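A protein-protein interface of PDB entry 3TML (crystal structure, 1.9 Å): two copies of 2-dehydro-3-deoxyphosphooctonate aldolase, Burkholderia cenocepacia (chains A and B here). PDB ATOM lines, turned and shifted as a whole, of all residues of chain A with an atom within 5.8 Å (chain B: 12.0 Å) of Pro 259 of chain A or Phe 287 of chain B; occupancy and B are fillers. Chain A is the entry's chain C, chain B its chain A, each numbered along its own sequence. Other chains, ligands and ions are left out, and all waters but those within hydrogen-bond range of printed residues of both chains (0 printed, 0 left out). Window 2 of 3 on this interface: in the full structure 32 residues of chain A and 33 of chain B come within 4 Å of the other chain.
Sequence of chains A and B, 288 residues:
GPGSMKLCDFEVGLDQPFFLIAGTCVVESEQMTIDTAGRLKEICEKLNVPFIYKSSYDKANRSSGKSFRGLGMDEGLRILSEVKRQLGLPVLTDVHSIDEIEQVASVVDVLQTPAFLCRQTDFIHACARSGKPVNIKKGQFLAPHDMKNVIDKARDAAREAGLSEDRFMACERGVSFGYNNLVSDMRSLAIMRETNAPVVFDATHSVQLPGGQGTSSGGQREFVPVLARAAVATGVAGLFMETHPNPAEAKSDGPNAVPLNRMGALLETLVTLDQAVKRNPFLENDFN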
ATOM      1  N   ARG A 221       4.367  30.658 -12.243  1.00  0.00           N
ATOM      2  CA  ARG A 221       5.342  30.247 -13.245  1.00  0.00           C
ATOM      3  C   ARG A 221       5.607  28.747 -13.235  1.00  0.00           C
ATOM      4  O   ARG A 221       5.797  28.160 -14.303  1.00  0.00           O
ATOM      5  CB  ARG A 221       6.670  30.994 -13.014  1.00  0.00           C
ATOM      6  CG  ARG A 221       7.744  30.667 -14.035  1.00  0.00           C
ATOM      7  CD  ARG A 221       9.057  31.389 -13.722  1.00  0.00           C
ATOM      8  NE  ARG A 221       8.858  32.831 -13.823  1.00  0.00           N
ATOM      9  CZ  ARG A 221       9.025  33.716 -12.840  1.00  0.00           C
ATOM     10  NH1 ARG A 221       9.461  33.351 -11.636  1.00  0.00           N
ATOM     11  NH2 ARG A 221       8.774  34.996 -13.082  1.00  0.00           N
ATOM     12  N   GLU A 222       5.605  28.141 -12.045  1.00  0.00           N
ATOM     13  CA  GLU A 222       5.951  26.724 -11.890  1.00  0.00           C
ATOM     14  C   GLU A 222       5.023  25.808 -12.689  1.00  0.00           C
ATOM     15  O   GLU A 222       5.438  24.736 -13.112  1.00  0.00           O
ATOM     16  CB  GLU A 222       6.018  26.297 -10.406  1.00  0.00           C
ATOM     17  CG  GLU A 222       4.735  26.471  -9.614  1.00  0.00           C
ATOM     18  CD  GLU A 222       4.708  25.712  -8.295  1.00  0.00           C
ATOM     19  OE1 GLU A 222       5.194  24.546  -8.241  1.00  0.00           O
ATOM     20  OE2 GLU A 222       4.150  26.270  -7.318  1.00  0.00           O
ATOM     21  N   PRO A 225       5.509  25.017 -17.351  1.00  0.00           N
ATOM     22  CA  PRO A 225       6.045  23.785 -17.976  1.00  0.00           C
ATOM     23  C   PRO A 225       5.098  22.599 -17.856  1.00  0.00           C
ATOM     24  O   PRO A 225       5.019  21.791 -18.778  1.00  0.00           O
ATOM     25  CB  PRO A 225       7.340  23.489 -17.201  1.00  0.00           C
ATOM     26  CG  PRO A 225       7.591  24.656 -16.296  1.00  0.00           C
ATOM     27  CD  PRO A 225       6.416  25.599 -16.337  1.00  0.00           C
ATOM     28  N   THR A 243       7.780  35.058 -22.517  1.00  0.00           N
ATOM     29  CA  THR A 243       9.134  34.922 -21.997  1.00  0.00           C
ATOM     30  C   THR A 243       9.753  36.288 -21.726  1.00  0.00           C
ATOM     31  O   THR A 243       9.232  37.295 -22.153  1.00  0.00           O
ATOM     32  CB  THR A 243      10.045  34.134 -22.975  1.00  0.00           C
ATOM     33  OG1 THR A 243      11.264  33.788 -22.310  1.00  0.00           O
ATOM     34  CG2 THR A 243      10.377  34.949 -24.206  1.00  0.00           C
ATOM     35  N   HIS A 244      10.879  36.304 -21.029  1.00  0.00           N
ATOM     36  CA  HIS A 244      11.587  37.550 -20.697  1.00  0.00           C
ATOM     37  C   HIS A 244      12.996  37.201 -20.290  1.00  0.00           C
ATOM     38  O   HIS A 244      13.218  36.139 -19.712  1.00  0.00           O
ATOM     39  CB  HIS A 244      10.862  38.298 -19.577  1.00  0.00           C
ATOM     40  CG  HIS A 244      11.266  39.761 -19.462  1.00  0.00           C
ATOM     41  ND1 HIS A 244      12.477  40.152 -19.000  1.00  0.00           N
ATOM     42  CD2 HIS A 244      10.571  40.938 -19.782  1.00  0.00           C
ATOM     43  CE1 HIS A 244      12.561  41.508 -19.040  1.00  0.00           C
ATOM     44  NE2 HIS A 244      11.396  41.987 -19.515  1.00  0.00           N
ATOM     45  N   PRO A 245      13.985  38.049 -20.612  1.00  0.00           N
ATOM     46  CA  PRO A 245      15.360  37.788 -20.127  1.00  0.00           C
ATOM     47  C   PRO A 245      15.492  37.664 -18.605  1.00  0.00           C
ATOM     48  O   PRO A 245      16.204  36.792 -18.124  1.00  0.00           O
ATOM     49  CB  PRO A 245      16.146  39.021 -20.591  1.00  0.00           C
ATOM     50  CG  PRO A 245      15.352  39.607 -21.693  1.00  0.00           C
ATOM     51  CD  PRO A 245      13.931  39.152 -21.593  1.00  0.00           C
ATOM     52  N   PRO A 247      12.452  37.881 -15.817  1.00  0.00           N
ATOM     53  CA  PRO A 247      11.064  38.086 -15.408  1.00  0.00           C
ATOM     54  C   PRO A 247      10.881  38.996 -14.169  1.00  0.00           C
ATOM     55  O   PRO A 247       9.922  39.771 -14.117  1.00  0.00           O
ATOM     56  CB  PRO A 247      10.590  36.665 -15.118  1.00  0.00           C
ATOM     57  CG  PRO A 247      11.371  35.813 -16.063  1.00  0.00           C
ATOM     58  CD  PRO A 247      12.723  36.462 -16.128  1.00  0.00           C
ATOM     59  N   ALA A 257       6.075  34.613 -16.672  1.00  0.00           N
ATOM     60  CA  ALA A 257       6.901  34.503 -17.871  1.00  0.00           C
ATOM     61  C   ALA A 257       7.957  33.425 -17.639  1.00  0.00           C
ATOM     62  O   ALA A 257       8.528  33.302 -16.546  1.00  0.00           O
ATOM     63  CB  ALA A 257       7.548  35.852 -18.205  1.00  0.00           C
ATOM     64  N   VAL A 258       8.242  32.642 -18.673  1.00  0.00           N
ATOM     65  CA  VAL A 258       9.353  31.691 -18.601  1.00  0.00           C
ATOM     66  C   VAL A 258      10.628  32.462 -18.885  1.00  0.00           C
ATOM     67  O   VAL A 258      10.669  33.250 -19.841  1.00  0.00           O
ATOM     68  CB  VAL A 258       9.165  30.531 -19.600  1.00  0.00           C
ATOM     69  CG1 VAL A 258      10.446  29.721 -19.736  1.00  0.00           C
ATOM     70  CG2 VAL A 258       8.009  29.649 -19.126  1.00  0.00           C
ATOM     71  N   PRO A 259      11.658  32.283 -18.034  1.00  0.00           N
ATOM     72  CA  PRO A 259      12.909  32.939 -18.330  1.00  0.00           C
ATOM     73  C   PRO A 259      13.458  32.485 -19.669  1.00  0.00           C
ATOM     74  O   PRO A 259      13.426  31.279 -20.008  1.00  0.00           O
ATOM     75  CB  PRO A 259      13.836  32.512 -17.177  1.00  0.00           C
ATOM     76  CG  PRO A 259      13.204  31.317 -16.571  1.00  0.00           C
ATOM     77  CD  PRO A 259      11.738  31.457 -16.816  1.00  0.00           C
ATOM     78  N   LEU A 260      13.958  33.457 -20.430  1.00  0.00           N
ATOM     79  CA  LEU A 260      14.505  33.200 -21.753  1.00  0.00           C
ATOM     80  C   LEU A 260      15.589  32.124 -21.731  1.00  0.00           C
ATOM     81  O   LEU A 260      15.598  31.275 -22.594  1.00  0.00           O
ATOM     82  CB  LEU A 260      15.013  34.528 -22.353  1.00  0.00           C
ATOM     83  CG  LEU A 260      15.420  34.610 -23.811  1.00  0.00           C
ATOM     84  CD1 LEU A 260      14.276  34.110 -24.675  1.00  0.00           C
ATOM     85  CD2 LEU A 260      15.832  36.058 -24.144  1.00  0.00           C
ATOM     86  N   ASN A 261      16.458  32.109 -20.720  1.00  0.00           N
ATOM     87  CA  ASN A 261      17.522  31.079 -20.632  1.00  0.00           C
ATOM     88  C   ASN A 261      17.052  29.639 -20.283  1.00  0.00           C
ATOM     89  O   ASN A 261      17.846  28.696 -20.274  1.00  0.00           O
ATOM     90  CB  ASN A 261      18.671  31.538 -19.720  1.00  0.00           C
ATOM     91  CG  ASN A 261      18.290  31.604 -18.257  1.00  0.00           C
ATOM     92  OD1 ASN A 261      17.190  31.216 -17.846  1.00  0.00           O
ATOM     93  ND2 ASN A 261      19.210  32.123 -17.453  1.00  0.00           N
ATOM     94  N   ARG A 262      15.762  29.460 -20.036  1.00  0.00           N
ATOM     95  CA  ARG A 262      15.197  28.122 -19.863  1.00  0.00           C
ATOM     96  C   ARG A 262      14.294  27.725 -21.057  1.00  0.00           C
ATOM     97  O   ARG A 262      13.760  26.606 -21.107  1.00  0.00           O
ATOM     98  CB  ARG A 262      14.460  28.073 -18.522  1.00  0.00           C
ATOM     99  N   MET A 263      14.114  28.623 -22.030  1.00  0.00           N
ATOM    100  CA  MET A 263      13.192  28.342 -23.130  1.00  0.00           C
ATOM    101  C   MET A 263      13.697  27.214 -23.999  1.00  0.00           C
ATOM    102  O   MET A 263      12.913  26.385 -24.443  1.00  0.00           O
ATOM    103  CB  MET A 263      12.912  29.594 -23.977  1.00  0.00           C
ATOM    104  CG  MET A 263      11.972  30.584 -23.301  1.00  0.00           C
ATOM    105  SD  MET A 263      10.252  30.027 -23.228  1.00  0.00           S
ATOM    106  CE  MET A 263       9.967  29.342 -24.848  1.00  0.00           C
ATOM    107  N   ALA B 190       1.270  17.780 -10.054  1.00  0.00           N
ATOM    108  CA  ALA B 190       2.510  18.421  -9.572  1.00  0.00           C
ATOM    109  C   ALA B 190       2.421  18.813  -8.088  1.00  0.00           C
ATOM    110  O   ALA B 190       3.360  18.548  -7.295  1.00  0.00           O
ATOM    111  CB  ALA B 190       2.868  19.639 -10.418  1.00  0.00           C
ATOM    112  N   ILE B 191       1.302  19.427  -7.694  1.00  0.00           N
ATOM    113  CA  ILE B 191       1.093  19.820  -6.313  1.00  0.00           C
ATOM    114  C   ILE B 191       1.206  18.639  -5.344  1.00  0.00           C
ATOM    115  O   ILE B 191       1.869  18.722  -4.325  1.00  0.00           O
ATOM    116  CB  ILE B 191      -0.281  20.525  -6.145  1.00  0.00           C
ATOM    117  CG1 ILE B 191      -0.286  21.871  -6.876  1.00  0.00           C
ATOM    118  CG2 ILE B 191      -0.560  20.793  -4.670  1.00  0.00           C
ATOM    119  CD1 ILE B 191      -1.672  22.451  -7.143  1.00  0.00           C
ATOM    120  N   ARG B 193       2.951  16.070  -5.358  1.00  0.00           N
ATOM    121  CA  ARG B 193       4.337  15.683  -5.051  1.00  0.00           C
ATOM    122  C   ARG B 193       4.773  16.122  -3.659  1.00  0.00           C
ATOM    123  O   ARG B 193       5.698  15.516  -3.056  1.00  0.00           O
ATOM    124  CB  ARG B 193       5.336  16.197  -6.115  1.00  0.00           C
ATOM    125  CG  ARG B 193       5.061  15.656  -7.508  1.00  0.00           C
ATOM    126  CD  ARG B 193       5.832  16.409  -8.581  1.00  0.00           C
ATOM    127  NE  ARG B 193       5.354  16.018  -9.901  1.00  0.00           N
ATOM    128  CZ  ARG B 193       5.659  16.642 -11.041  1.00  0.00           C
ATOM    129  NH1 ARG B 193       6.464  17.697 -11.048  1.00  0.00           N
ATOM    130  NH2 ARG B 193       5.155  16.193 -12.186  1.00  0.00           N
ATOM    131  N   PRO B 281      15.666  16.691 -15.503  1.00  0.00           N
ATOM    132  CA  PRO B 281      14.872  17.257 -14.407  1.00  0.00           C
ATOM    133  C   PRO B 281      13.571  17.957 -14.892  1.00  0.00           C
ATOM    134  O   PRO B 281      13.511  18.478 -16.008  1.00  0.00           O
ATOM    135  CB  PRO B 281      15.836  18.271 -13.771  1.00  0.00           C
ATOM    136  CG  PRO B 281      17.181  17.684 -14.024  1.00  0.00           C
ATOM    137  CD  PRO B 281      17.082  17.099 -15.413  1.00  0.00           C
ATOM    138  N   PHE B 282      12.529  17.933 -14.076  1.00  0.00           N
ATOM    139  CA  PHE B 282      11.310  18.641 -14.424  1.00  0.00           C
ATOM    140  C   PHE B 282      11.608  20.119 -14.284  1.00  0.00           C
ATOM    141  O   PHE B 282      12.118  20.553 -13.251  1.00  0.00           O
ATOM    142  CB  PHE B 282      10.158  18.224 -13.524  1.00  0.00           C
ATOM    143  CG  PHE B 282       9.639  16.844 -13.803  1.00  0.00           C
ATOM    144  CD1 PHE B 282       8.849  16.602 -14.919  1.00  0.00           C
ATOM    145  CD2 PHE B 282       9.905  15.787 -12.931  1.00  0.00           C
ATOM    146  CE1 PHE B 282       8.338  15.346 -15.179  1.00  0.00           C
ATOM    147  CE2 PHE B 282       9.411  14.508 -13.189  1.00  0.00           C
ATOM    148  CZ  PHE B 282       8.615  14.292 -14.314  1.00  0.00           C
ATOM    149  N   LEU B 283      11.319  20.892 -15.330  1.00  0.00           N
ATOM    150  CA  LEU B 283      11.626  22.325 -15.287  1.00  0.00           C
ATOM    151  C   LEU B 283      10.900  23.089 -14.173  1.00  0.00           C
ATOM    152  O   LEU B 283      11.422  24.080 -13.668  1.00  0.00           O
ATOM    153  CB  LEU B 283      11.343  22.972 -16.657  1.00  0.00           C
ATOM    154  CG  LEU B 283      11.775  24.417 -16.808  1.00  0.00           C
ATOM    155  CD1 LEU B 283      13.300  24.529 -16.683  1.00  0.00           C
ATOM    156  CD2 LEU B 283      11.240  25.017 -18.108  1.00  0.00           C
ATOM    157  N   GLU B 284       9.708  22.647 -13.776  1.00  0.00           N
ATOM    158  CA  GLU B 284       8.995  23.308 -12.654  1.00  0.00           C
ATOM    159  C   GLU B 284       9.785  23.318 -11.334  1.00  0.00           C
ATOM    160  O   GLU B 284       9.545  24.157 -10.467  1.00  0.00           O
ATOM    161  CB  GLU B 284       7.629  22.690 -12.397  1.00  0.00           C
ATOM    162  CG  GLU B 284       7.621  21.188 -12.152  1.00  0.00           C
ATOM    163  CD  GLU B 284       7.389  20.395 -13.427  1.00  0.00           C
ATOM    164  OE1 GLU B 284       7.873  20.818 -14.534  1.00  0.00           O
ATOM    165  OE2 GLU B 284       6.734  19.351 -13.331  1.00  0.00           O
ATOM    166  N   ASN B 285      10.688  22.368 -11.167  1.00  0.00           N
ATOM    167  CA  ASN B 285      11.564  22.345  -9.997  1.00  0.00           C
ATOM    168  C   ASN B 285      12.600  23.494  -9.965  1.00  0.00           C
ATOM    169  O   ASN B 285      13.158  23.751  -8.921  1.00  0.00           O
ATOM    170  CB  ASN B 285      12.241  20.972  -9.867  1.00  0.00           C
ATOM    171  CG  ASN B 285      11.247  19.858  -9.524  1.00  0.00           C
ATOM    172  OD1 ASN B 285      10.162  20.110  -9.005  1.00  0.00           O
ATOM    173  ND2 ASN B 285      11.615  18.627  -9.827  1.00  0.00           N
ATOM    174  N   ASP B 286      12.853  24.174 -11.089  1.00  0.00           N
ATOM    175  CA  ASP B 286      13.648  25.420 -11.084  1.00  0.00           C
ATOM    176  C   ASP B 286      12.827  26.672 -10.752  1.00  0.00           C
ATOM    177  O   ASP B 286      13.410  27.728 -10.479  1.00  0.00           O
ATOM    178  CB  ASP B 286      14.318  25.671 -12.435  1.00  0.00           C
ATOM    179  CG  ASP B 286      15.411  24.682 -12.741  1.00  0.00           C
ATOM    180  OD1 ASP B 286      15.774  23.878 -11.846  1.00  0.00           O
ATOM    181  OD2 ASP B 286      15.906  24.711 -13.894  1.00  0.00           O
ATOM    182  N   PHE B 287      11.492  26.579 -10.816  1.00  0.00           N
ATOM    183  CA  PHE B 287      10.611  27.694 -10.428  1.00  0.00           C
ATOM    184  C   PHE B 287       9.756  27.285  -9.223  1.00  0.00           C
ATOM    185  O   PHE B 287       9.085  28.123  -8.616  1.00  0.00           O
ATOM    186  CB  PHE B 287       9.712  28.148 -11.591  1.00  0.00           C
ATOM    187  CG  PHE B 287      10.348  28.021 -12.960  1.00  0.00           C
ATOM    188  CD1 PHE B 287      11.656  28.421 -13.185  1.00  0.00           C
ATOM    189  CD2 PHE B 287       9.609  27.532 -14.038  1.00  0.00           C
ATOM    190  CE1 PHE B 287      12.219  28.302 -14.443  1.00  0.00           C
ATOM    191  CE2 PHE B 287      10.160  27.430 -15.298  1.00  0.00           C
ATOM    192  CZ  PHE B 287      11.468  27.804 -15.499  1.00  0.00           C
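Pro 259 of chain A touches one residue of chain B. Of the printed residues of chain A, Phe 287 of chain B touches Arg 221, Glu 222, Pro 225 and Pro 259. Of chain B, only Phe 287 (3.6 Å) comes within 4 Å of Arg 221 of chain A. No residue of chain B comes within 4 Å of Pro 245 of chain A. No residue of chain B comes within 4 Å of Asn 261 of chain A. No residue of chain B comes within 4 Å of Arg 262 of chain A. No residue of chain B comes within 4 Å of Met 263 of chain A. Of the printed residues of chain B, Pro 225 of chain A touches Glu 284 and Phe 287. Printed residues of chain B within 4 Å of Glu 222 of chain A: Glu 284 and Phe 287. His 244 of chain A touches none of the printed residues of chain B. The nearest residue of chain B that does not touch Pro 259 of chain A is Leu 283 of chain B (6.6 Å). The nearest printed residue of chain B that does not touch Pro 225 of chain A is Leu 283 of chain B (4.1 Å).
Among the printed residues, merely in contact across the chains: Arg 221 of chain A with Phe 287 of chain B, Glu 222 of chain A with Glu 284 of chain B, Glu 222 of chain A with Phe 287 of chain B, Pro 225 of chain A with Glu 284 of chain B, Pro 225 of chain A with Phe 287 of chain B and Pro 259 of chain A with Phe 287 of chain B.
Hydrophobic or aromatic side chains of chain A within 4 Å of the printed part of chain B: Pro 225 and Pro 259. Hydrophobic or aromatic side chains of chain B that line the printed part of chain A: Phe 287. Among the printed residues, 6 pairs touch across the chains.
The guanidinium group (NE) of Arg 221 of chain A sits at hydrogen-bond distance from the backbone carbonyl oxygen (O) of Ala 257 of chain A, at 2.8 Å. The guanidinium group (NH1) of Arg 193 of chain B lies within salt-bridge range of the side-chain carboxylate (OE2) of Glu 284 of chain B.
No position is printed for both chains.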
